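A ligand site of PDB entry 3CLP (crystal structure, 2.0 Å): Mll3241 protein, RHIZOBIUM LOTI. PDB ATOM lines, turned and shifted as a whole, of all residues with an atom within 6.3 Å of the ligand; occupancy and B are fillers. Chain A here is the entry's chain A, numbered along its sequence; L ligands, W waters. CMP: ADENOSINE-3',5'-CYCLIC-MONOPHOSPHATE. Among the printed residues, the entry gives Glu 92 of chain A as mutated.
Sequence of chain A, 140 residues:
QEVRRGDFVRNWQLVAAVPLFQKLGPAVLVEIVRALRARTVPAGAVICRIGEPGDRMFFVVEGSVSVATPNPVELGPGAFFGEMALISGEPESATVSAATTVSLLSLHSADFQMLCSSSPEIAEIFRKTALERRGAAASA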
ATOM      1  N   CYS A  48      16.494  11.137 -22.993  1.00  0.00           N
ATOM      2  CA  CYS A  48      15.365  12.014 -23.286  1.00  0.00           C
ATOM      3  C   CYS A  48      15.838  13.430 -23.575  1.00  0.00           C
ATOM      4  O   CYS A  48      16.899  13.846 -23.109  1.00  0.00           O
ATOM      5  CB  CYS A  48      14.321  11.970 -22.160  1.00  0.00           C
ATOM      6  SG  CYS A  48      14.902  12.555 -20.557  1.00  0.00           S
ATOM      7  N   GLY A  54       6.794  14.105 -22.546  1.00  0.00           N
ATOM      8  CA  GLY A  54       7.176  12.959 -21.737  1.00  0.00           C
ATOM      9  C   GLY A  54       6.109  11.888 -21.730  1.00  0.00           C
ATOM     10  O   GLY A  54       5.034  12.091 -21.179  1.00  0.00           O
ATOM     11  N   ARG A  56       7.079   8.659 -20.832  1.00  0.00           N
ATOM     12  CA  ARG A  56       7.636   7.656 -19.926  1.00  0.00           C
ATOM     13  C   ARG A  56       8.691   8.222 -18.976  1.00  0.00           C
ATOM     14  O   ARG A  56       9.266   9.274 -19.234  1.00  0.00           O
ATOM     15  CB  ARG A  56       8.237   6.482 -20.727  1.00  0.00           C
ATOM     16  CG  ARG A  56       9.534   6.800 -21.454  1.00  0.00           C
ATOM     17  CD  ARG A  56       9.810   5.813 -22.560  1.00  0.00           C
ATOM     18  NE  ARG A  56       8.846   5.943 -23.648  1.00  0.00           N
ATOM     19  CZ  ARG A  56       8.769   5.135 -24.693  1.00  0.00           C
ATOM     20  NH1 ARG A  56       9.610   4.104 -24.827  1.00  0.00           N
ATOM     21  NH2 ARG A  56       7.843   5.342 -25.618  1.00  0.00           N
ATOM     22  N   VAL A  67      21.985  14.863 -16.182  1.00  0.00           N
ATOM     23  CA  VAL A  67      20.874  15.766 -16.458  1.00  0.00           C
ATOM     24  C   VAL A  67      21.456  17.116 -16.865  1.00  0.00           C
ATOM     25  O   VAL A  67      22.205  17.732 -16.104  1.00  0.00           O
ATOM     26  CB  VAL A  67      19.955  15.944 -15.222  1.00  0.00           C
ATOM     27  CG1 VAL A  67      18.761  16.825 -15.581  1.00  0.00           C
ATOM     28  CG2 VAL A  67      19.504  14.598 -14.690  1.00  0.00           C
ATOM     29  N   THR A  69      20.832  20.250 -16.841  1.00  0.00           N
ATOM     30  CA  THR A  69      20.447  21.526 -16.226  1.00  0.00           C
ATOM     31  C   THR A  69      21.652  22.478 -16.340  1.00  0.00           C
ATOM     32  O   THR A  69      22.760  22.005 -16.587  1.00  0.00           O
ATOM     33  CB  THR A  69      20.035  21.345 -14.739  1.00  0.00           C
ATOM     34  OG1 THR A  69      20.916  20.394 -14.113  1.00  0.00           O
ATOM     35  CG2 THR A  69      18.606  20.836 -14.640  1.00  0.00           C
ATOM     36  N   ASN A  71      23.503  23.780 -14.188  1.00  0.00           N
ATOM     37  CA  ASN A  71      24.505  23.084 -13.414  1.00  0.00           C
ATOM     38  C   ASN A  71      24.136  21.600 -13.419  1.00  0.00           C
ATOM     39  O   ASN A  71      23.294  21.178 -12.626  1.00  0.00           O
ATOM     40  CB  ASN A  71      24.559  23.646 -11.994  1.00  0.00           C
ATOM     41  CG  ASN A  71      24.977  25.116 -11.968  1.00  0.00           C
ATOM     42  OD1 ASN A  71      26.135  25.452 -12.220  1.00  0.00           O
ATOM     43  ND2 ASN A  71      24.012  25.991 -11.683  1.00  0.00           N
ATOM     44  N   VAL A  73      23.438  17.624 -13.223  1.00  0.00           N
ATOM     45  CA  VAL A  73      23.375  16.701 -12.084  1.00  0.00           C
ATOM     46  C   VAL A  73      23.546  15.272 -12.565  1.00  0.00           C
ATOM     47  O   VAL A  73      22.864  14.850 -13.514  1.00  0.00           O
ATOM     48  CB  VAL A  73      22.030  16.844 -11.312  1.00  0.00           C
ATOM     49  CG1 VAL A  73      21.991  15.904 -10.092  1.00  0.00           C
ATOM     50  CG2 VAL A  73      21.794  18.295 -10.882  1.00  0.00           C
ATOM     51  N   LEU A  75      22.939  11.480 -11.849  1.00  0.00           N
ATOM     52  CA  LEU A  75      22.093  10.573 -11.080  1.00  0.00           C
ATOM     53  C   LEU A  75      22.590   9.132 -11.126  1.00  0.00           C
ATOM     54  O   LEU A  75      22.930   8.628 -12.193  1.00  0.00           O
ATOM     55  CB  LEU A  75      20.637  10.668 -11.549  1.00  0.00           C
ATOM     56  CG  LEU A  75      19.998  12.065 -11.494  1.00  0.00           C
ATOM     57  CD1 LEU A  75      18.593  12.060 -12.114  1.00  0.00           C
ATOM     58  CD2 LEU A  75      19.951  12.606 -10.076  1.00  0.00           C
ATOM     59  N   PHE A  80      15.683   8.164 -10.215  1.00  0.00           N
ATOM     60  CA  PHE A  80      14.715   8.178 -11.289  1.00  0.00           C
ATOM     61  C   PHE A  80      14.696   9.541 -11.959  1.00  0.00           C
ATOM     62  O   PHE A  80      15.050  10.545 -11.341  1.00  0.00           O
ATOM     63  CB  PHE A  80      13.324   7.812 -10.765  1.00  0.00           C
ATOM     64  CG  PHE A  80      12.844   8.691  -9.638  1.00  0.00           C
ATOM     65  CD1 PHE A  80      12.338   9.960  -9.887  1.00  0.00           C
ATOM     66  CD2 PHE A  80      12.903   8.242  -8.324  1.00  0.00           C
ATOM     67  CE1 PHE A  80      11.904  10.787  -8.849  1.00  0.00           C
ATOM     68  CE2 PHE A  80      12.468   9.055  -7.270  1.00  0.00           C
ATOM     69  CZ  PHE A  80      11.964  10.328  -7.538  1.00  0.00           C
ATOM     70  N   PHE A  81      14.266   9.577 -13.219  1.00  0.00           N
ATOM     71  CA  PHE A  81      14.152  10.818 -13.985  1.00  0.00           C
ATOM     72  C   PHE A  81      13.084  10.689 -15.067  1.00  0.00           C
ATOM     73  O   PHE A  81      12.809   9.589 -15.565  1.00  0.00           O
ATOM     74  CB  PHE A  81      15.502  11.225 -14.606  1.00  0.00           C
ATOM     75  CG  PHE A  81      16.058  10.231 -15.577  1.00  0.00           C
ATOM     76  CD1 PHE A  81      15.767  10.320 -16.937  1.00  0.00           C
ATOM     77  CD2 PHE A  81      16.894   9.190 -15.149  1.00  0.00           C
ATOM     78  CE1 PHE A  81      16.291   9.406 -17.852  1.00  0.00           C
ATOM     79  CE2 PHE A  81      17.426   8.274 -16.053  1.00  0.00           C
ATOM     80  CZ  PHE A  81      17.125   8.383 -17.410  1.00  0.00           C
ATOM     81  N   GLY A  82      12.485  11.820 -15.435  1.00  0.00           N
ATOM     82  CA  GLY A  82      11.388  11.847 -16.383  1.00  0.00           C
ATOM     83  C   GLY A  82      10.049  11.995 -15.681  1.00  0.00           C
ATOM     84  O   GLY A  82       9.007  11.996 -16.322  1.00  0.00           O
ATOM     85  N   GLU A  83      10.094  12.105 -14.349  1.00  0.00           N
ATOM     86  CA  GLU A  83       8.887  12.209 -13.534  1.00  0.00           C
ATOM     87  C   GLU A  83       8.208  13.583 -13.610  1.00  0.00           C
ATOM     88  O   GLU A  83       6.992  13.667 -13.456  1.00  0.00           O
ATOM     89  CB  GLU A  83       9.186  11.861 -12.065  1.00  0.00           C
ATOM     90  CG  GLU A  83       9.773  12.997 -11.205  1.00  0.00           C
ATOM     91  CD  GLU A  83      11.203  13.384 -11.587  1.00  0.00           C
ATOM     92  OE1 GLU A  83      11.866  12.628 -12.333  1.00  0.00           O
ATOM     93  OE2 GLU A  83      11.680  14.429 -11.115  1.00  0.00           O
ATOM     94  N   MET A  84       8.983  14.642 -13.849  1.00  0.00           N
ATOM     95  CA  MET A  84       8.428  16.000 -13.846  1.00  0.00           C
ATOM     96  C   MET A  84       7.374  16.220 -14.933  1.00  0.00           C
ATOM     97  O   MET A  84       6.305  16.759 -14.658  1.00  0.00           O
ATOM     98  CB  MET A  84       9.533  17.050 -13.947  1.00  0.00           C
ATOM     99  CG  MET A  84      10.418  17.125 -12.717  1.00  0.00           C
ATOM    100  SD  MET A  84      11.835  18.206 -12.950  1.00  0.00           S
ATOM    101  CE  MET A  84      11.041  19.801 -13.059  1.00  0.00           C
ATOM    102  N   ALA A  85       7.687  15.781 -16.152  1.00  0.00           N
ATOM    103  CA  ALA A  85       6.766  15.889 -17.283  1.00  0.00           C
ATOM    104  C   ALA A  85       5.514  15.058 -17.065  1.00  0.00           C
ATOM    105  O   ALA A  85       4.404  15.488 -17.423  1.00  0.00           O
ATOM    106  CB  ALA A  85       7.456  15.456 -18.573  1.00  0.00           C
ATOM    107  N   LEU A  86       5.672  13.877 -16.477  1.00  0.00           N
ATOM    108  CA  LEU A  86       4.544  12.990 -16.188  1.00  0.00           C
ATOM    109  C   LEU A  86       3.623  13.551 -15.116  1.00  0.00           C
ATOM    110  O   LEU A  86       2.426  13.270 -15.122  1.00  0.00           O
ATOM    111  CB  LEU A  86       5.026  11.585 -15.787  1.00  0.00           C
ATOM    112  CG  LEU A  86       5.780  10.747 -16.810  1.00  0.00           C
ATOM    113  CD1 LEU A  86       6.079   9.349 -16.258  1.00  0.00           C
ATOM    114  CD2 LEU A  86       5.011  10.648 -18.117  1.00  0.00           C
ATOM    115  N   GLU A  90       3.741  18.975 -18.742  1.00  0.00           N
ATOM    116  CA  GLU A  90       4.589  19.857 -19.537  1.00  0.00           C
ATOM    117  C   GLU A  90       5.699  19.084 -20.239  1.00  0.00           C
ATOM    118  O   GLU A  90       5.968  17.918 -19.906  1.00  0.00           O
ATOM    119  CB  GLU A  90       5.194  20.938 -18.656  1.00  0.00           C
ATOM    120  CG  GLU A  90       4.178  21.962 -18.210  1.00  0.00           C
ATOM    121  CD  GLU A  90       4.712  22.829 -17.104  1.00  0.00           C
ATOM    122  OE1 GLU A  90       5.421  23.799 -17.409  1.00  0.00           O
ATOM    123  OE2 GLU A  90       4.404  22.522 -15.933  1.00  0.00           O
ATOM    124  N   PRO A  91       6.378  19.721 -21.225  1.00  0.00           N
ATOM    125  CA  PRO A  91       7.484  19.025 -21.860  1.00  0.00           C
ATOM    126  C   PRO A  91       8.669  18.764 -20.915  1.00  0.00           C
ATOM    127  O   PRO A  91       8.826  19.423 -19.896  1.00  0.00           O
ATOM    128  CB  PRO A  91       7.888  19.989 -22.993  1.00  0.00           C
ATOM    129  CG  PRO A  91       6.701  20.838 -23.204  1.00  0.00           C
ATOM    130  CD  PRO A  91       6.123  21.050 -21.840  1.00  0.00           C
ATOM    131  N   GLU A  92       9.456  17.749 -21.266  1.00  0.00           N
ATOM    132  CA  GLU A  92      10.738  17.457 -20.648  1.00  0.00           C
ATOM    133  C   GLU A  92      11.514  18.730 -20.368  1.00  0.00           C
ATOM    134  O   GLU A  92      11.727  19.522 -21.277  1.00  0.00           O
ATOM    135  CB  GLU A  92      11.540  16.606 -21.660  1.00  0.00           C
ATOM    136  CG  GLU A  92      11.724  15.158 -21.302  1.00  0.00           C
ATOM    137  CD  GLU A  92      10.653  14.314 -21.965  1.00  0.00           C
ATOM    138  OE1 GLU A  92       9.433  14.563 -21.724  1.00  0.00           O
ATOM    139  OE2 GLU A  92      10.982  13.355 -22.721  1.00  0.00           O
ATOM    140  N   SER A  93      11.870  18.892 -19.030  1.00  0.00           N
ATOM    141  CA  SER A  93      12.515  20.137 -18.624  1.00  0.00           C
ATOM    142  C   SER A  93      14.008  20.196 -18.959  1.00  0.00           C
ATOM    143  O   SER A  93      14.601  21.278 -18.931  1.00  0.00           O
ATOM    144  CB  SER A  93      12.278  20.414 -17.125  1.00  0.00           C
ATOM    145  OG  SER A  93      12.934  19.443 -16.317  1.00  0.00           O
ATOM    146  N   ALA A  94      14.612  19.053 -19.291  1.00  0.00           N
ATOM    147  CA  ALA A  94      16.059  18.960 -19.582  1.00  0.00           C
ATOM    148  C   ALA A  94      16.397  17.700 -20.372  1.00  0.00           C
ATOM    149  O   ALA A  94      15.668  16.713 -20.318  1.00  0.00           O
ATOM    150  CB  ALA A  94      16.857  18.987 -18.277  1.00  0.00           C
ATOM    151  N   THR A  95      17.501  17.744 -21.113  1.00  0.00           N
ATOM    152  CA  THR A  95      18.032  16.584 -21.793  1.00  0.00           C
ATOM    153  C   THR A  95      18.730  15.707 -20.755  1.00  0.00           C
ATOM    154  O   THR A  95      19.440  16.218 -19.887  1.00  0.00           O
ATOM    155  CB  THR A  95      19.011  16.979 -22.930  1.00  0.00           C
ATOM    156  OG1 THR A  95      18.291  17.633 -23.977  1.00  0.00           O
ATOM    157  CG2 THR A  95      19.723  15.755 -23.497  1.00  0.00           C
ATOM    158  N   VAL A  96      18.489  14.403 -20.833  1.00  0.00           N
ATOM    159  CA  VAL A  96      19.180  13.450 -19.967  1.00  0.00           C
ATOM    160  C   VAL A  96      19.929  12.454 -20.830  1.00  0.00           C
ATOM    161  O   VAL A  96      19.363  11.853 -21.747  1.00  0.00           O
ATOM    162  CB  VAL A  96      18.219  12.711 -18.985  1.00  0.00           C
ATOM    163  CG1 VAL A  96      19.012  11.865 -17.995  1.00  0.00           C
ATOM    164  CG2 VAL A  96      17.338  13.708 -18.226  1.00  0.00           C
ATOM    165  N   GLU A 132      11.239  19.778  -5.644  1.00  0.00           N
ATOM    166  CA  GLU A 132      12.624  20.015  -5.242  1.00  0.00           C
ATOM    167  C   GLU A 132      13.518  20.302  -6.450  1.00  0.00           C
ATOM    168  O   GLU A 132      14.435  21.120  -6.381  1.00  0.00           O
ATOM    169  CB  GLU A 132      13.130  18.788  -4.481  1.00  0.00           C
ATOM    170  CG  GLU A 132      14.201  19.061  -3.409  1.00  0.00           C
ATOM    171  CD  GLU A 132      14.393  17.841  -2.498  1.00  0.00           C
ATOM    172  OE1 GLU A 132      14.400  16.695  -3.014  1.00  0.00           O
ATOM    173  OE2 GLU A 132      14.538  18.036  -1.273  1.00  0.00           O
ATOM    174  N   ARG A 133      13.226  19.620  -7.557  1.00  0.00           N
ATOM    175  CA  ARG A 133      13.981  19.782  -8.805  1.00  0.00           C
ATOM    176  C   ARG A 133      13.550  21.001  -9.622  1.00  0.00           C
ATOM    177  O   ARG A 133      14.350  21.558 -10.379  1.00  0.00           O
ATOM    178  CB  ARG A 133      13.892  18.503  -9.655  1.00  0.00           C
ATOM    179  CG  ARG A 133      14.682  17.361  -9.047  1.00  0.00           C
ATOM    180  CD  ARG A 133      14.482  16.042  -9.761  1.00  0.00           C
ATOM    181  NE  ARG A 133      15.419  15.059  -9.220  1.00  0.00           N
ATOM    182  CZ  ARG A 133      15.427  13.773  -9.519  1.00  0.00           C
ATOM    183  NH1 ARG A 133      14.525  13.266 -10.362  1.00  0.00           N
ATOM    184  NH2 ARG A 133      16.336  12.973  -8.971  1.00  0.00           N
ATOM    185  N   ARG A 134      12.297  21.428  -9.449  1.00  0.00           N
ATOM    186  CA  ARG A 134      11.765  22.607 -10.129  1.00  0.00           C
ATOM    187  C   ARG A 134      12.358  23.899  -9.563  1.00  0.00           C
ATOM    188  O   ARG A 134      12.481  24.039  -8.321  1.00  0.00           O
ATOM    189  CB  ARG A 134      10.234  22.642 -10.043  1.00  0.00           C
HETATM  190  P   CMP L   1      11.332  15.667 -16.963  1.00  0.00           P
HETATM  191  O1P CMP L   1      11.129  17.166 -16.941  1.00  0.00           O
HETATM  192  O2P CMP L   1      10.064  14.922 -17.282  1.00  0.00           O
HETATM  193  O5' CMP L   1      12.506  15.328 -18.017  1.00  0.00           O
HETATM  194  C5' CMP L   1      13.863  15.754 -17.730  1.00  0.00           C
HETATM  195  C4' CMP L   1      14.237  15.161 -16.360  1.00  0.00           C
HETATM  196  O4' CMP L   1      15.515  15.565 -15.837  1.00  0.00           O
HETATM  197  C3' CMP L   1      13.266  15.654 -15.306  1.00  0.00           C
HETATM  198  O3' CMP L   1      11.936  15.152 -15.567  1.00  0.00           O
HETATM  199  C2' CMP L   1      13.940  15.263 -14.011  1.00  0.00           C
HETATM  200  O2' CMP L   1      13.804  13.855 -13.795  1.00  0.00           O
HETATM  201  C1' CMP L   1      15.419  15.567 -14.387  1.00  0.00           C
HETATM  202  N9  CMP L   1      15.727  16.897 -13.764  1.00  0.00           N
HETATM  203  C8  CMP L   1      15.252  18.105 -14.157  1.00  0.00           C
HETATM  204  N7  CMP L   1      15.711  19.098 -13.348  1.00  0.00           N
HETATM  205  C5  CMP L   1      16.492  18.523 -12.423  1.00  0.00           C
HETATM  206  C6  CMP L   1      17.298  18.970 -11.262  1.00  0.00           C
HETATM  207  N6  CMP L   1      17.367  20.288 -10.919  1.00  0.00           N
HETATM  208  N1  CMP L   1      17.971  18.040 -10.546  1.00  0.00           N
HETATM  209  C2  CMP L   1      17.929  16.726 -10.856  1.00  0.00           C
HETATM  210  N3  CMP L   1      17.232  16.228 -11.875  1.00  0.00           N
HETATM  211  C4  CMP L   1      16.495  17.066 -12.688  1.00  0.00           C
HETATM  212  O   HOH W   1      16.340  22.826 -12.218  1.00  0.00           O
HETATM  213  O   HOH W   2       9.005  12.342 -18.998  1.00  0.00           O
HETATM  214  O   HOH W   3      18.725  18.383  -8.007  1.00  0.00           O
HETATM  215  O   HOH W   4       8.984  18.721 -17.222  1.00  0.00           O
HETATM  216  O   HOH W   5      14.848  21.610 -14.331  1.00  0.00           O
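The side-chain carboxylate (OE2) of Glu 83 is in salt-bridge range of the guanidinium group (NH1) of Arg 133 (3.2 Å).
The side-chain hydroxyl of Ser 93 is in hydrogen-bond range of the side-chain sulfur of Met 84, at 3.8 Å.
NH1 of Arg 133 sits at hydrogen-bond distance from O of Phe 80, at 2.9 Å.
The side-chain carboxylate (OE1) of Glu 92 sits close to the backbone NH (N) of Gly 54 (2.8 Å).
N of Val 67 sits at hydrogen-bond distance from O of Val 73, at 2.8 Å.
O of Cys 48 sits at hydrogen-bond distance from N of Val 96, 2.8 Å away.
O of Asn 71 is in hydrogen-bond range of OG1 of Thr 69, at 2.9 Å.
OE1 of Glu 83 lies within hydrogen-bond range of O2' of the ligand (2.7 Å).
O2P of the ligand sits at hydrogen-bond distance from N of Ala 85 (2.8 Å).
N of Ser 93 lies within hydrogen-bond range of O1P of the ligand.
OG of Ser 93 sits at hydrogen-bond distance from O1P of the ligand.
N of Gly 82 sits at hydrogen-bond distance from O2' of the ligand.
N6 of the ligand sits at hydrogen-bond distance from O of Arg 133 (3.3 Å).
The guanidinium group (NE) of Arg 133 sits at hydrogen-bond distance from a nitrogen (N3) of the ligand, at 3.4 Å.
The backbone NH of Met 84 sits at hydrogen-bond distance from an oxygen (O3') of the ligand.
Water W4 lies within hydrogen-bond range of an oxygen (O1P) of the ligand, the backbone carbonyl oxygen of Pro 91, the backbone NH of Ala 85 and the backbone NH of Ser 93.
Water W1 bridges O of Arg 133 (3.0 Å) and N6 of the ligand (3.0 Å).
Water W2 lies within hydrogen-bond range of O of Gly 82 (2.7 Å), O of Arg 56 (3.1 Å) and O2P of the ligand (3.3 Å).
Merely in contact with the ligand: Phe 81 (3.1 Å), Ala 94 (3.3 Å), Glu 92 (3.4 Å), Val 67 (3.5 Å), Val 96 (3.5 Å), Thr 69 (3.6 Å) and Val 73 (3.8 Å).
Within 4 Å of the ligand: Val 67, Thr 69, Val 73, Phe 81, Gly 82, Glu 83, Met 84, Ala 85, Glu 92, Ser 93, Ala 94, Val 96 and Arg 133.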
